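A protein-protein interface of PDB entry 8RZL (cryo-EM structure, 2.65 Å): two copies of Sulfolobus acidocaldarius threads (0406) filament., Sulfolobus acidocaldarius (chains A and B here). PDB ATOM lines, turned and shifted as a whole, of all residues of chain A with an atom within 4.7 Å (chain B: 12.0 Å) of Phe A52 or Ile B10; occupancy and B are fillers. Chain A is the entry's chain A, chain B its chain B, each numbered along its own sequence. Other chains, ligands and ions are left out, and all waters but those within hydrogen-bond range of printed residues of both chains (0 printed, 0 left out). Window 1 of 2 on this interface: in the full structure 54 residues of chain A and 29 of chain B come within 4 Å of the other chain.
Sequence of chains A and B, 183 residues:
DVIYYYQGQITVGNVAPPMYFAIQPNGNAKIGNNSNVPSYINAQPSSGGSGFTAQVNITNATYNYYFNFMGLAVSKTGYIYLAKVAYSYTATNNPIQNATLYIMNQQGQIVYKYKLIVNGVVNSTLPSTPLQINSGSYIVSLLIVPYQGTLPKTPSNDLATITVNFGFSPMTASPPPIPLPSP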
ATOM      1  N   PHE A  21     -10.308  36.427  -5.737  1.00  0.00           N
ATOM      2  CA  PHE A  21     -11.475  35.879  -6.407  1.00  0.00           C
ATOM      3  C   PHE A  21     -12.406  37.016  -6.819  1.00  0.00           C
ATOM      4  O   PHE A  21     -12.600  37.969  -6.062  1.00  0.00           O
ATOM      5  CB  PHE A  21     -12.154  34.851  -5.505  1.00  0.00           C
ATOM      6  CG  PHE A  21     -11.335  33.604  -5.288  1.00  0.00           C
ATOM      7  CD1 PHE A  21     -10.385  33.539  -4.278  1.00  0.00           C
ATOM      8  CD2 PHE A  21     -11.497  32.498  -6.113  1.00  0.00           C
ATOM      9  CE1 PHE A  21      -9.631  32.390  -4.081  1.00  0.00           C
ATOM     10  CE2 PHE A  21     -10.738  31.350  -5.921  1.00  0.00           C
ATOM     11  CZ  PHE A  21      -9.804  31.299  -4.907  1.00  0.00           C
ATOM     12  N   GLN A  44     -20.536  33.746  -4.892  1.00  0.00           N
ATOM     13  CA  GLN A  44     -20.111  35.133  -4.796  1.00  0.00           C
ATOM     14  C   GLN A  44     -18.668  35.188  -4.305  1.00  0.00           C
ATOM     15  O   GLN A  44     -18.236  34.323  -3.542  1.00  0.00           O
ATOM     16  CB  GLN A  44     -21.021  35.908  -3.840  1.00  0.00           C
ATOM     17  CG  GLN A  44     -22.366  36.294  -4.447  1.00  0.00           C
ATOM     18  CD  GLN A  44     -23.209  37.190  -3.569  1.00  0.00           C
ATOM     19  OE1 GLN A  44     -22.948  37.368  -2.380  1.00  0.00           O
ATOM     20  NE2 GLN A  44     -24.247  37.766  -4.157  1.00  0.00           N
ATOM     21  N   PRO A  45     -17.885  36.223  -4.682  1.00  0.00           N
ATOM     22  CA  PRO A  45     -16.581  36.422  -4.063  1.00  0.00           C
ATOM     23  C   PRO A  45     -16.824  36.928  -2.643  1.00  0.00           C
ATOM     24  O   PRO A  45     -17.720  37.743  -2.410  1.00  0.00           O
ATOM     25  CB  PRO A  45     -15.906  37.475  -4.950  1.00  0.00           C
ATOM     26  CG  PRO A  45     -17.048  38.250  -5.578  1.00  0.00           C
ATOM     27  CD  PRO A  45     -18.238  37.315  -5.604  1.00  0.00           C
ATOM     28  N   SER A  46     -16.051  36.394  -1.691  1.00  0.00           N
ATOM     29  CA  SER A  46     -16.057  36.879  -0.319  1.00  0.00           C
ATOM     30  C   SER A  46     -15.542  38.320  -0.286  1.00  0.00           C
ATOM     31  O   SER A  46     -14.884  38.756  -1.227  1.00  0.00           O
ATOM     32  CB  SER A  46     -15.257  35.968   0.572  1.00  0.00           C
ATOM     33  OG  SER A  46     -15.418  36.336   1.932  1.00  0.00           O
ATOM     34  N   GLY A  51     -11.636  35.367  -0.976  1.00  0.00           N
ATOM     35  CA  GLY A  51     -12.098  33.985  -1.007  1.00  0.00           C
ATOM     36  C   GLY A  51     -13.441  33.924  -1.726  1.00  0.00           C
ATOM     37  O   GLY A  51     -13.792  34.878  -2.411  1.00  0.00           O
ATOM     38  N   PHE A  52     -14.206  32.842  -1.536  1.00  0.00           N
ATOM     39  CA  PHE A  52     -15.522  32.756  -2.157  1.00  0.00           C
ATOM     40  C   PHE A  52     -16.498  31.957  -1.295  1.00  0.00           C
ATOM     41  O   PHE A  52     -16.099  31.122  -0.485  1.00  0.00           O
ATOM     42  CB  PHE A  52     -15.423  32.190  -3.577  1.00  0.00           C
ATOM     43  CG  PHE A  52     -14.968  30.753  -3.657  1.00  0.00           C
ATOM     44  CD1 PHE A  52     -15.885  29.710  -3.587  1.00  0.00           C
ATOM     45  CD2 PHE A  52     -13.624  30.441  -3.812  1.00  0.00           C
ATOM     46  CE1 PHE A  52     -15.467  28.388  -3.658  1.00  0.00           C
ATOM     47  CE2 PHE A  52     -13.208  29.118  -3.887  1.00  0.00           C
ATOM     48  CZ  PHE A  52     -14.129  28.094  -3.808  1.00  0.00           C
ATOM     49  N   THR A  53     -17.793  32.214  -1.515  1.00  0.00           N
ATOM     50  CA  THR A  53     -18.874  31.478  -0.877  1.00  0.00           C
ATOM     51  C   THR A  53     -19.782  30.938  -1.977  1.00  0.00           C
ATOM     52  O   THR A  53     -20.114  31.675  -2.897  1.00  0.00           O
ATOM     53  CB  THR A  53     -19.673  32.383   0.071  1.00  0.00           C
ATOM     54  OG1 THR A  53     -18.804  32.934   1.061  1.00  0.00           O
ATOM     55  CG2 THR A  53     -20.829  31.682   0.755  1.00  0.00           C
ATOM     56  N   ALA A  54     -20.177  29.663  -1.877  1.00  0.00           N
ATOM     57  CA  ALA A  54     -21.051  29.059  -2.878  1.00  0.00           C
ATOM     58  C   ALA A  54     -22.136  28.193  -2.238  1.00  0.00           C
ATOM     59  O   ALA A  54     -21.848  27.406  -1.337  1.00  0.00           O
ATOM     60  CB  ALA A  54     -20.229  28.266  -3.865  1.00  0.00           C
ATOM     61  N   VAL A  56     -24.617  25.302  -3.593  1.00  0.00           N
ATOM     62  CA  VAL A  56     -24.463  24.422  -4.740  1.00  0.00           C
ATOM     63  C   VAL A  56     -25.476  23.291  -4.615  1.00  0.00           C
ATOM     64  O   VAL A  56     -25.424  22.510  -3.666  1.00  0.00           O
ATOM     65  CB  VAL A  56     -23.019  23.890  -4.823  1.00  0.00           C
ATOM     66  CG1 VAL A  56     -22.856  22.793  -5.851  1.00  0.00           C
ATOM     67  CG2 VAL A  56     -22.018  24.993  -5.104  1.00  0.00           C
ATOM     68  N   PHE A  69     -17.783  28.967 -12.211  1.00  0.00           N
ATOM     69  CA  PHE A  69     -18.616  29.580 -11.179  1.00  0.00           C
ATOM     70  C   PHE A  69     -17.924  30.760 -10.487  1.00  0.00           C
ATOM     71  O   PHE A  69     -18.585  31.558  -9.824  1.00  0.00           O
ATOM     72  CB  PHE A  69     -19.086  28.532 -10.167  1.00  0.00           C
ATOM     73  CG  PHE A  69     -18.050  28.126  -9.145  1.00  0.00           C
ATOM     74  CD1 PHE A  69     -17.932  28.813  -7.944  1.00  0.00           C
ATOM     75  CD2 PHE A  69     -17.185  27.062  -9.382  1.00  0.00           C
ATOM     76  CE1 PHE A  69     -16.972  28.457  -7.005  1.00  0.00           C
ATOM     77  CE2 PHE A  69     -16.228  26.700  -8.443  1.00  0.00           C
ATOM     78  CZ  PHE A  69     -16.126  27.395  -7.253  1.00  0.00           C
ATOM     79  N   MET A  70     -16.589  30.841 -10.595  1.00  0.00           N
ATOM     80  CA  MET A  70     -15.782  31.919 -10.037  1.00  0.00           C
ATOM     81  C   MET A  70     -14.662  32.262 -11.019  1.00  0.00           C
ATOM     82  O   MET A  70     -14.326  31.467 -11.896  1.00  0.00           O
ATOM     83  CB  MET A  70     -15.165  31.510  -8.695  1.00  0.00           C
ATOM     84  CG  MET A  70     -15.939  31.966  -7.478  1.00  0.00           C
ATOM     85  SD  MET A  70     -15.941  33.767  -7.255  1.00  0.00           S
ATOM     86  CE  MET A  70     -17.653  34.118  -7.646  1.00  0.00           C
ATOM     87  N   LEU A 101     -11.799  20.372  -7.528  1.00  0.00           N
ATOM     88  CA  LEU A 101     -11.828  21.790  -7.842  1.00  0.00           C
ATOM     89  C   LEU A 101     -10.697  22.081  -8.830  1.00  0.00           C
ATOM     90  O   LEU A 101      -9.559  21.692  -8.593  1.00  0.00           O
ATOM     91  CB  LEU A 101     -11.665  22.516  -6.502  1.00  0.00           C
ATOM     92  CG  LEU A 101     -11.777  24.039  -6.466  1.00  0.00           C
ATOM     93  CD1 LEU A 101     -13.005  24.529  -7.209  1.00  0.00           C
ATOM     94  CD2 LEU A 101     -11.860  24.498  -5.022  1.00  0.00           C
ATOM     95  N   LEU A 116     -10.490  17.503  -3.454  1.00  0.00           N
ATOM     96  CA  LEU A 116     -10.886  17.913  -2.112  1.00  0.00           C
ATOM     97  C   LEU A 116     -11.304  16.693  -1.290  1.00  0.00           C
ATOM     98  O   LEU A 116     -10.904  16.536  -0.135  1.00  0.00           O
ATOM     99  CB  LEU A 116     -12.040  18.921  -2.188  1.00  0.00           C
ATOM    100  CG  LEU A 116     -11.858  20.133  -3.105  1.00  0.00           C
ATOM    101  CD1 LEU A 116     -13.108  20.995  -3.077  1.00  0.00           C
ATOM    102  CD2 LEU A 116     -10.640  20.956  -2.720  1.00  0.00           C
ATOM    103  N   LEU A 142     -16.010  23.494 -10.261  1.00  0.00           N
ATOM    104  CA  LEU A 142     -16.152  22.443  -9.262  1.00  0.00           C
ATOM    105  C   LEU A 142     -16.895  21.241  -9.851  1.00  0.00           C
ATOM    106  O   LEU A 142     -17.927  21.403 -10.491  1.00  0.00           O
ATOM    107  CB  LEU A 142     -16.899  23.048  -8.069  1.00  0.00           C
ATOM    108  CG  LEU A 142     -17.289  22.098  -6.940  1.00  0.00           C
ATOM    109  CD1 LEU A 142     -16.070  21.650  -6.143  1.00  0.00           C
ATOM    110  CD2 LEU A 142     -18.295  22.774  -6.025  1.00  0.00           C
ATOM    111  N   ALA A 160     -24.576  19.142   3.072  1.00  0.00           N
ATOM    112  CA  ALA A 160     -23.151  19.072   3.385  1.00  0.00           C
ATOM    113  C   ALA A 160     -22.476  20.439   3.244  1.00  0.00           C
ATOM    114  O   ALA A 160     -23.023  21.356   2.633  1.00  0.00           O
ATOM    115  CB  ALA A 160     -22.470  18.035   2.521  1.00  0.00           C
ATOM    116  N   THR A 161     -21.273  20.566   3.822  1.00  0.00           N
ATOM    117  CA  THR A 161     -20.456  21.765   3.689  1.00  0.00           C
ATOM    118  C   THR A 161     -18.993  21.378   3.473  1.00  0.00           C
ATOM    119  O   THR A 161     -18.481  20.491   4.152  1.00  0.00           O
ATOM    120  CB  THR A 161     -20.681  22.757   4.843  1.00  0.00           C
ATOM    121  OG1 THR A 161     -19.816  23.879   4.662  1.00  0.00           O
ATOM    122  CG2 THR A 161     -20.451  22.165   6.218  1.00  0.00           C
ATOM    123  N   ILE A 162     -18.342  22.045   2.510  1.00  0.00           N
ATOM    124  CA  ILE A 162     -16.923  21.884   2.233  1.00  0.00           C
ATOM    125  C   ILE A 162     -16.250  23.237   2.437  1.00  0.00           C
ATOM    126  O   ILE A 162     -16.632  24.217   1.802  1.00  0.00           O
ATOM    127  CB  ILE A 162     -16.682  21.362   0.798  1.00  0.00           C
ATOM    128  CG1 ILE A 162     -17.522  20.124   0.468  1.00  0.00           C
ATOM    129  CG2 ILE A 162     -15.194  21.137   0.550  1.00  0.00           C
ATOM    130  CD1 ILE A 162     -17.522  19.728  -0.995  1.00  0.00           C
ATOM    131  N   VAL A 164     -12.503  25.056   2.123  1.00  0.00           N
ATOM    132  CA  VAL A 164     -11.219  24.851   1.472  1.00  0.00           C
ATOM    133  C   VAL A 164     -10.362  26.109   1.621  1.00  0.00           C
ATOM    134  O   VAL A 164     -10.855  27.215   1.438  1.00  0.00           O
ATOM    135  CB  VAL A 164     -11.391  24.423  -0.002  1.00  0.00           C
ATOM    136  CG1 VAL A 164     -12.368  25.297  -0.782  1.00  0.00           C
ATOM    137  CG2 VAL A 164     -10.060  24.383  -0.721  1.00  0.00           C
ATOM    138  N   TYR B   4      -0.215  33.866   1.885  1.00  0.00           N
ATOM    139  CA  TYR B   4      -1.555  34.415   1.980  1.00  0.00           C
ATOM    140  C   TYR B   4      -2.546  33.283   1.733  1.00  0.00           C
ATOM    141  O   TYR B   4      -2.447  32.601   0.716  1.00  0.00           O
ATOM    142  CB  TYR B   4      -1.713  35.583   1.002  1.00  0.00           C
ATOM    143  CG  TYR B   4      -0.824  36.763   1.304  1.00  0.00           C
ATOM    144  CD1 TYR B   4      -1.007  37.520   2.454  1.00  0.00           C
ATOM    145  CD2 TYR B   4       0.209  37.128   0.450  1.00  0.00           C
ATOM    146  CE1 TYR B   4      -0.195  38.607   2.747  1.00  0.00           C
ATOM    147  CE2 TYR B   4       1.036  38.207   0.731  1.00  0.00           C
ATOM    148  CZ  TYR B   4       0.831  38.954   1.882  1.00  0.00           C
ATOM    149  OH  TYR B   4       1.637  40.022   2.163  1.00  0.00           O
ATOM    150  N   TYR B   5      -3.498  33.094   2.655  1.00  0.00           N
ATOM    151  CA  TYR B   5      -4.493  32.043   2.512  1.00  0.00           C
ATOM    152  C   TYR B   5      -5.869  32.626   2.194  1.00  0.00           C
ATOM    153  O   TYR B   5      -6.313  33.585   2.828  1.00  0.00           O
ATOM    154  CB  TYR B   5      -4.564  31.184   3.771  1.00  0.00           C
ATOM    155  CG  TYR B   5      -3.291  30.484   4.174  1.00  0.00           C
ATOM    156  CD1 TYR B   5      -2.981  29.220   3.693  1.00  0.00           C
ATOM    157  CD2 TYR B   5      -2.423  31.053   5.093  1.00  0.00           C
ATOM    158  CE1 TYR B   5      -1.830  28.552   4.090  1.00  0.00           C
ATOM    159  CE2 TYR B   5      -1.277  30.391   5.516  1.00  0.00           C
ATOM    160  CZ  TYR B   5      -0.971  29.137   5.007  1.00  0.00           C
ATOM    161  OH  TYR B   5       0.160  28.475   5.404  1.00  0.00           O
ATOM    162  N   TYR B   6      -6.529  32.000   1.211  1.00  0.00           N
ATOM    163  CA  TYR B   6      -7.837  32.392   0.706  1.00  0.00           C
ATOM    164  C   TYR B   6      -8.813  31.249   0.964  1.00  0.00           C
ATOM    165  O   TYR B   6      -8.539  30.108   0.593  1.00  0.00           O
ATOM    166  CB  TYR B   6      -7.747  32.723  -0.787  1.00  0.00           C
ATOM    167  CG  TYR B   6      -6.728  33.780  -1.128  1.00  0.00           C
ATOM    168  CD1 TYR B   6      -5.373  33.477  -1.169  1.00  0.00           C
ATOM    169  CD2 TYR B   6      -7.111  35.085  -1.401  1.00  0.00           C
ATOM    170  CE1 TYR B   6      -4.422  34.442  -1.456  1.00  0.00           C
ATOM    171  CE2 TYR B   6      -6.171  36.062  -1.701  1.00  0.00           C
ATOM    172  CZ  TYR B   6      -4.823  35.739  -1.737  1.00  0.00           C
ATOM    173  OH  TYR B   6      -3.884  36.689  -2.032  1.00  0.00           O
ATOM    174  N   GLN B   7      -9.953  31.562   1.593  1.00  0.00           N
ATOM    175  CA  GLN B   7     -10.882  30.531   2.030  1.00  0.00           C
ATOM    176  C   GLN B   7     -12.097  30.464   1.104  1.00  0.00           C
ATOM    177  O   GLN B   7     -12.840  31.433   0.967  1.00  0.00           O
ATOM    178  CB  GLN B   7     -11.284  30.758   3.488  1.00  0.00           C
ATOM    179  CG  GLN B   7     -12.068  29.601   4.085  1.00  0.00           C
ATOM    180  CD  GLN B   7     -12.201  29.746   5.579  1.00  0.00           C
ATOM    181  OE1 GLN B   7     -11.304  29.386   6.339  1.00  0.00           O
ATOM    182  NE2 GLN B   7     -13.334  30.275   6.011  1.00  0.00           N
ATOM    183  N   GLY B   8     -12.297  29.292   0.490  1.00  0.00           N
ATOM    184  CA  GLY B   8     -13.534  28.970  -0.197  1.00  0.00           C
ATOM    185  C   GLY B   8     -14.439  28.153   0.717  1.00  0.00           C
ATOM    186  O   GLY B   8     -13.995  27.182   1.328  1.00  0.00           O
ATOM    187  N   GLN B   9     -15.706  28.563   0.824  1.00  0.00           N
ATOM    188  CA  GLN B   9     -16.682  27.790   1.575  1.00  0.00           C
ATOM    189  C   GLN B   9     -17.840  27.398   0.660  1.00  0.00           C
ATOM    190  O   GLN B   9     -18.544  28.262   0.146  1.00  0.00           O
ATOM    191  CB  GLN B   9     -17.139  28.554   2.817  1.00  0.00           C
ATOM    192  CG  GLN B   9     -18.146  27.775   3.653  1.00  0.00           C
ATOM    193  CD  GLN B   9     -18.459  28.395   4.996  1.00  0.00           C
ATOM    194  OE1 GLN B   9     -17.677  29.164   5.551  1.00  0.00           O
ATOM    195  NE2 GLN B   9     -19.617  28.048   5.538  1.00  0.00           N
ATOM    196  N   ILE B  10     -18.029  26.085   0.481  1.00  0.00           N
ATOM    197  CA  ILE B  10     -19.055  25.545  -0.394  1.00  0.00           C
ATOM    198  C   ILE B  10     -20.083  24.827   0.478  1.00  0.00           C
ATOM    199  O   ILE B  10     -19.742  23.872   1.168  1.00  0.00           O
ATOM    200  CB  ILE B  10     -18.430  24.600  -1.443  1.00  0.00           C
ATOM    201  CG1 ILE B  10     -17.384  25.301  -2.317  1.00  0.00           C
ATOM    202  CG2 ILE B  10     -19.509  23.928  -2.285  1.00  0.00           C
ATOM    203  CD1 ILE B  10     -16.273  24.395  -2.799  1.00  0.00           C
ATOM    204  N   THR B  11     -21.339  25.289   0.430  1.00  0.00           N
ATOM    205  CA  THR B  11     -22.436  24.611   1.105  1.00  0.00           C
ATOM    206  C   THR B  11     -23.268  23.866   0.067  1.00  0.00           C
ATOM    207  O   THR B  11     -23.635  24.429  -0.960  1.00  0.00           O
ATOM    208  CB  THR B  11     -23.255  25.562   1.989  1.00  0.00           C
ATOM    209  OG1 THR B  11     -23.818  26.605   1.191  1.00  0.00           O
ATOM    210  CG2 THR B  11     -22.438  26.152   3.117  1.00  0.00           C
ATOM    211  N   VAL B  12     -23.535  22.586   0.347  1.00  0.00           N
ATOM    212  CA  VAL B  12     -24.121  21.686  -0.629  1.00  0.00           C
ATOM    213  C   VAL B  12     -25.554  21.365  -0.216  1.00  0.00           C
ATOM    214  O   VAL B  12     -25.794  20.883   0.888  1.00  0.00           O
ATOM    215  CB  VAL B  12     -23.266  20.417  -0.808  1.00  0.00           C
ATOM    216  CG1 VAL B  12     -23.910  19.412  -1.752  1.00  0.00           C
ATOM    217  CG2 VAL B  12     -21.858  20.757  -1.274  1.00  0.00           C
ATOM    218  N   GLY B  13     -26.488  21.656  -1.126  1.00  0.00           N
ATOM    219  CA  GLY B  13     -27.883  21.274  -0.985  1.00  0.00           C
ATOM    220  C   GLY B  13     -28.285  20.235  -2.029  1.00  0.00           C
ATOM    221  O   GLY B  13     -27.458  19.786  -2.819  1.00  0.00           O
ATOM    222  N   ASN B  14     -29.577  19.896  -2.045  1.00  0.00           N
ATOM    223  CA  ASN B  14     -30.090  18.797  -2.846  1.00  0.00           C
ATOM    224  C   ASN B  14     -31.355  19.247  -3.578  1.00  0.00           C
ATOM    225  O   ASN B  14     -32.236  19.833  -2.953  1.00  0.00           O
ATOM    226  CB  ASN B  14     -30.311  17.573  -1.950  1.00  0.00           C
ATOM    227  CG  ASN B  14     -31.253  16.555  -2.551  1.00  0.00           C
ATOM    228  OD1 ASN B  14     -30.997  16.034  -3.632  1.00  0.00           O
ATOM    229  ND2 ASN B  14     -32.337  16.261  -1.854  1.00  0.00           N
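The backbone NH (N) of Ile A162 sits at hydrogen-bond distance from the backbone carbonyl oxygen (O) of Ile B10 (2.7 Å). The backbone NH of Val B12 sits at hydrogen-bond distance from the backbone carbonyl oxygen of Ala A160 (2.6 Å). The backbone NH (N) of Ala A54 is in hydrogen-bond range of the backbone carbonyl oxygen (O) of Gln B9 (3.0 Å). OG1 of Thr A161 lies close to O of Ile B10, 3.5 Å away. O of Val A164 sits at hydrogen-bond distance from N of Gly B8. The backbone NH of Gly B13 is in hydrogen-bond range of the backbone carbonyl oxygen of Val A56, 2.9 Å away. N of Thr B11 lies within hydrogen-bond range of O of Ala A54, 2.8 Å away. The backbone NH (N) of Val A56 sits at hydrogen-bond distance from the backbone carbonyl oxygen (O) of Thr B11, 2.9 Å away. The backbone carbonyl oxygen (O) of Phe A52 is in hydrogen-bond range of the backbone NH (N) of Gln B9 (2.9 Å). O of Gln B7 is in hydrogen-bond range of N of Phe A52, at 3.2 Å.
No position is printed for both chains.
Printed residues of chain A that touch a printed residue of chain B: Phe A21, Gly A51, Phe A52, Thr A53, Ala A54, Val A56, Ala A160, Thr A161, Ile A162 and Val A164. Hydrophobic or aromatic side chains of chain A within 4 Å of the printed part of chain B: Phe A21, Phe A52, Val A56, Ile A162 and Val A164. Of the 11 printed residues of chain B, 8 touch a printed residue of chain A. Among the printed residues, no Asp or Glu carboxylate lies within 4 Å of a Lys or Arg side-chain nitrogen of the other chain.
Phe A52 touches four residues of chain B. Of the printed residues of chain A, Ile B10 touches Phe A52 (3.9 Å), Ala A54 (3.5 Å), Val A56 (3.9 Å), Thr A161 (3.4 Å) and Ile A162 (2.7 Å). Phe A21 touches just one residue of chain B: Tyr B6 (3.8 Å). No residue of chain B comes within 4 Å of Pro A45. No residue of chain B comes within 4 Å of Ser A46. Of chain B, only Gln B7 (3.3 Å) comes within 4 Å of Gly A51. Of chain B, only Gln B9 comes within 4 Å of Thr A53. Ala A54 touches just these residues of chain B: Gln B9, Ile B10 and Thr B11. Of chain B, only Ile B10, Thr B11, Val B12 and Gly B13 come within 4 Å of Val A56. Ala A160 touches just these residues of chain B: Thr B11 (3.6 Å) and Val B12 (2.6 Å). Of chain B, only Ile B10 (3.4 Å) and Thr B11 (3.8 Å) come within 4 Å of Thr A161. Printed residues of chain B within 4 Å of Ile A162: Gly B8 (3.996 Å), Gln B9 (3.6 Å) and Ile B10 (2.7 Å). Of the printed residues of chain A, Gln B9 touches Phe A52, Thr A53, Ala A54 and Ile A162. Printed residues of chain A within 4 Å of Gln B7: Gly A51 (3.3 Å), Phe A52 (3.2 Å) and Val A164 (3.4 Å). Of the printed residues of chain A, Val B12 touches Val A56 (3.4 Å) and Ala A160 (2.6 Å). Met A70 touches none of the printed residues of chain B. The nearest residue of chain B that does not touch Phe A52 is Tyr B6 (6.2 Å). The nearest printed residue of chain A that does not touch Gln B7 is Ser A46 (5.2 Å).
Tyr B6 touches Phe A21 (CB to CE1, 3.8 Å). CA of Gly A51 touches O of Gln B7, 3.3 Å away. O of Phe A52 touches CA of Gly B8, 3.4 Å away. Thr A53 touches Gln B9. Ile B10 touches Val A56 (CG2 to CG2, 3.9 Å). Val A56 touches Val B12. Ala A160 touches Thr B11 (O to C, 3.6 Å). Ile A162 touches Gly B8. Gln B9 touches Ile A162. Val A164 touches Tyr B6 (O to O, 3.8 Å).
The backbone NH (N) of Gln A44 lies within hydrogen-bond range of the backbone carbonyl oxygen (O) of Thr A53, at 2.9 Å. The backbone NH (N) of Ser A46 lies within hydrogen-bond range of the backbone carbonyl oxygen (O) of Gly A51, at 2.8 Å.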
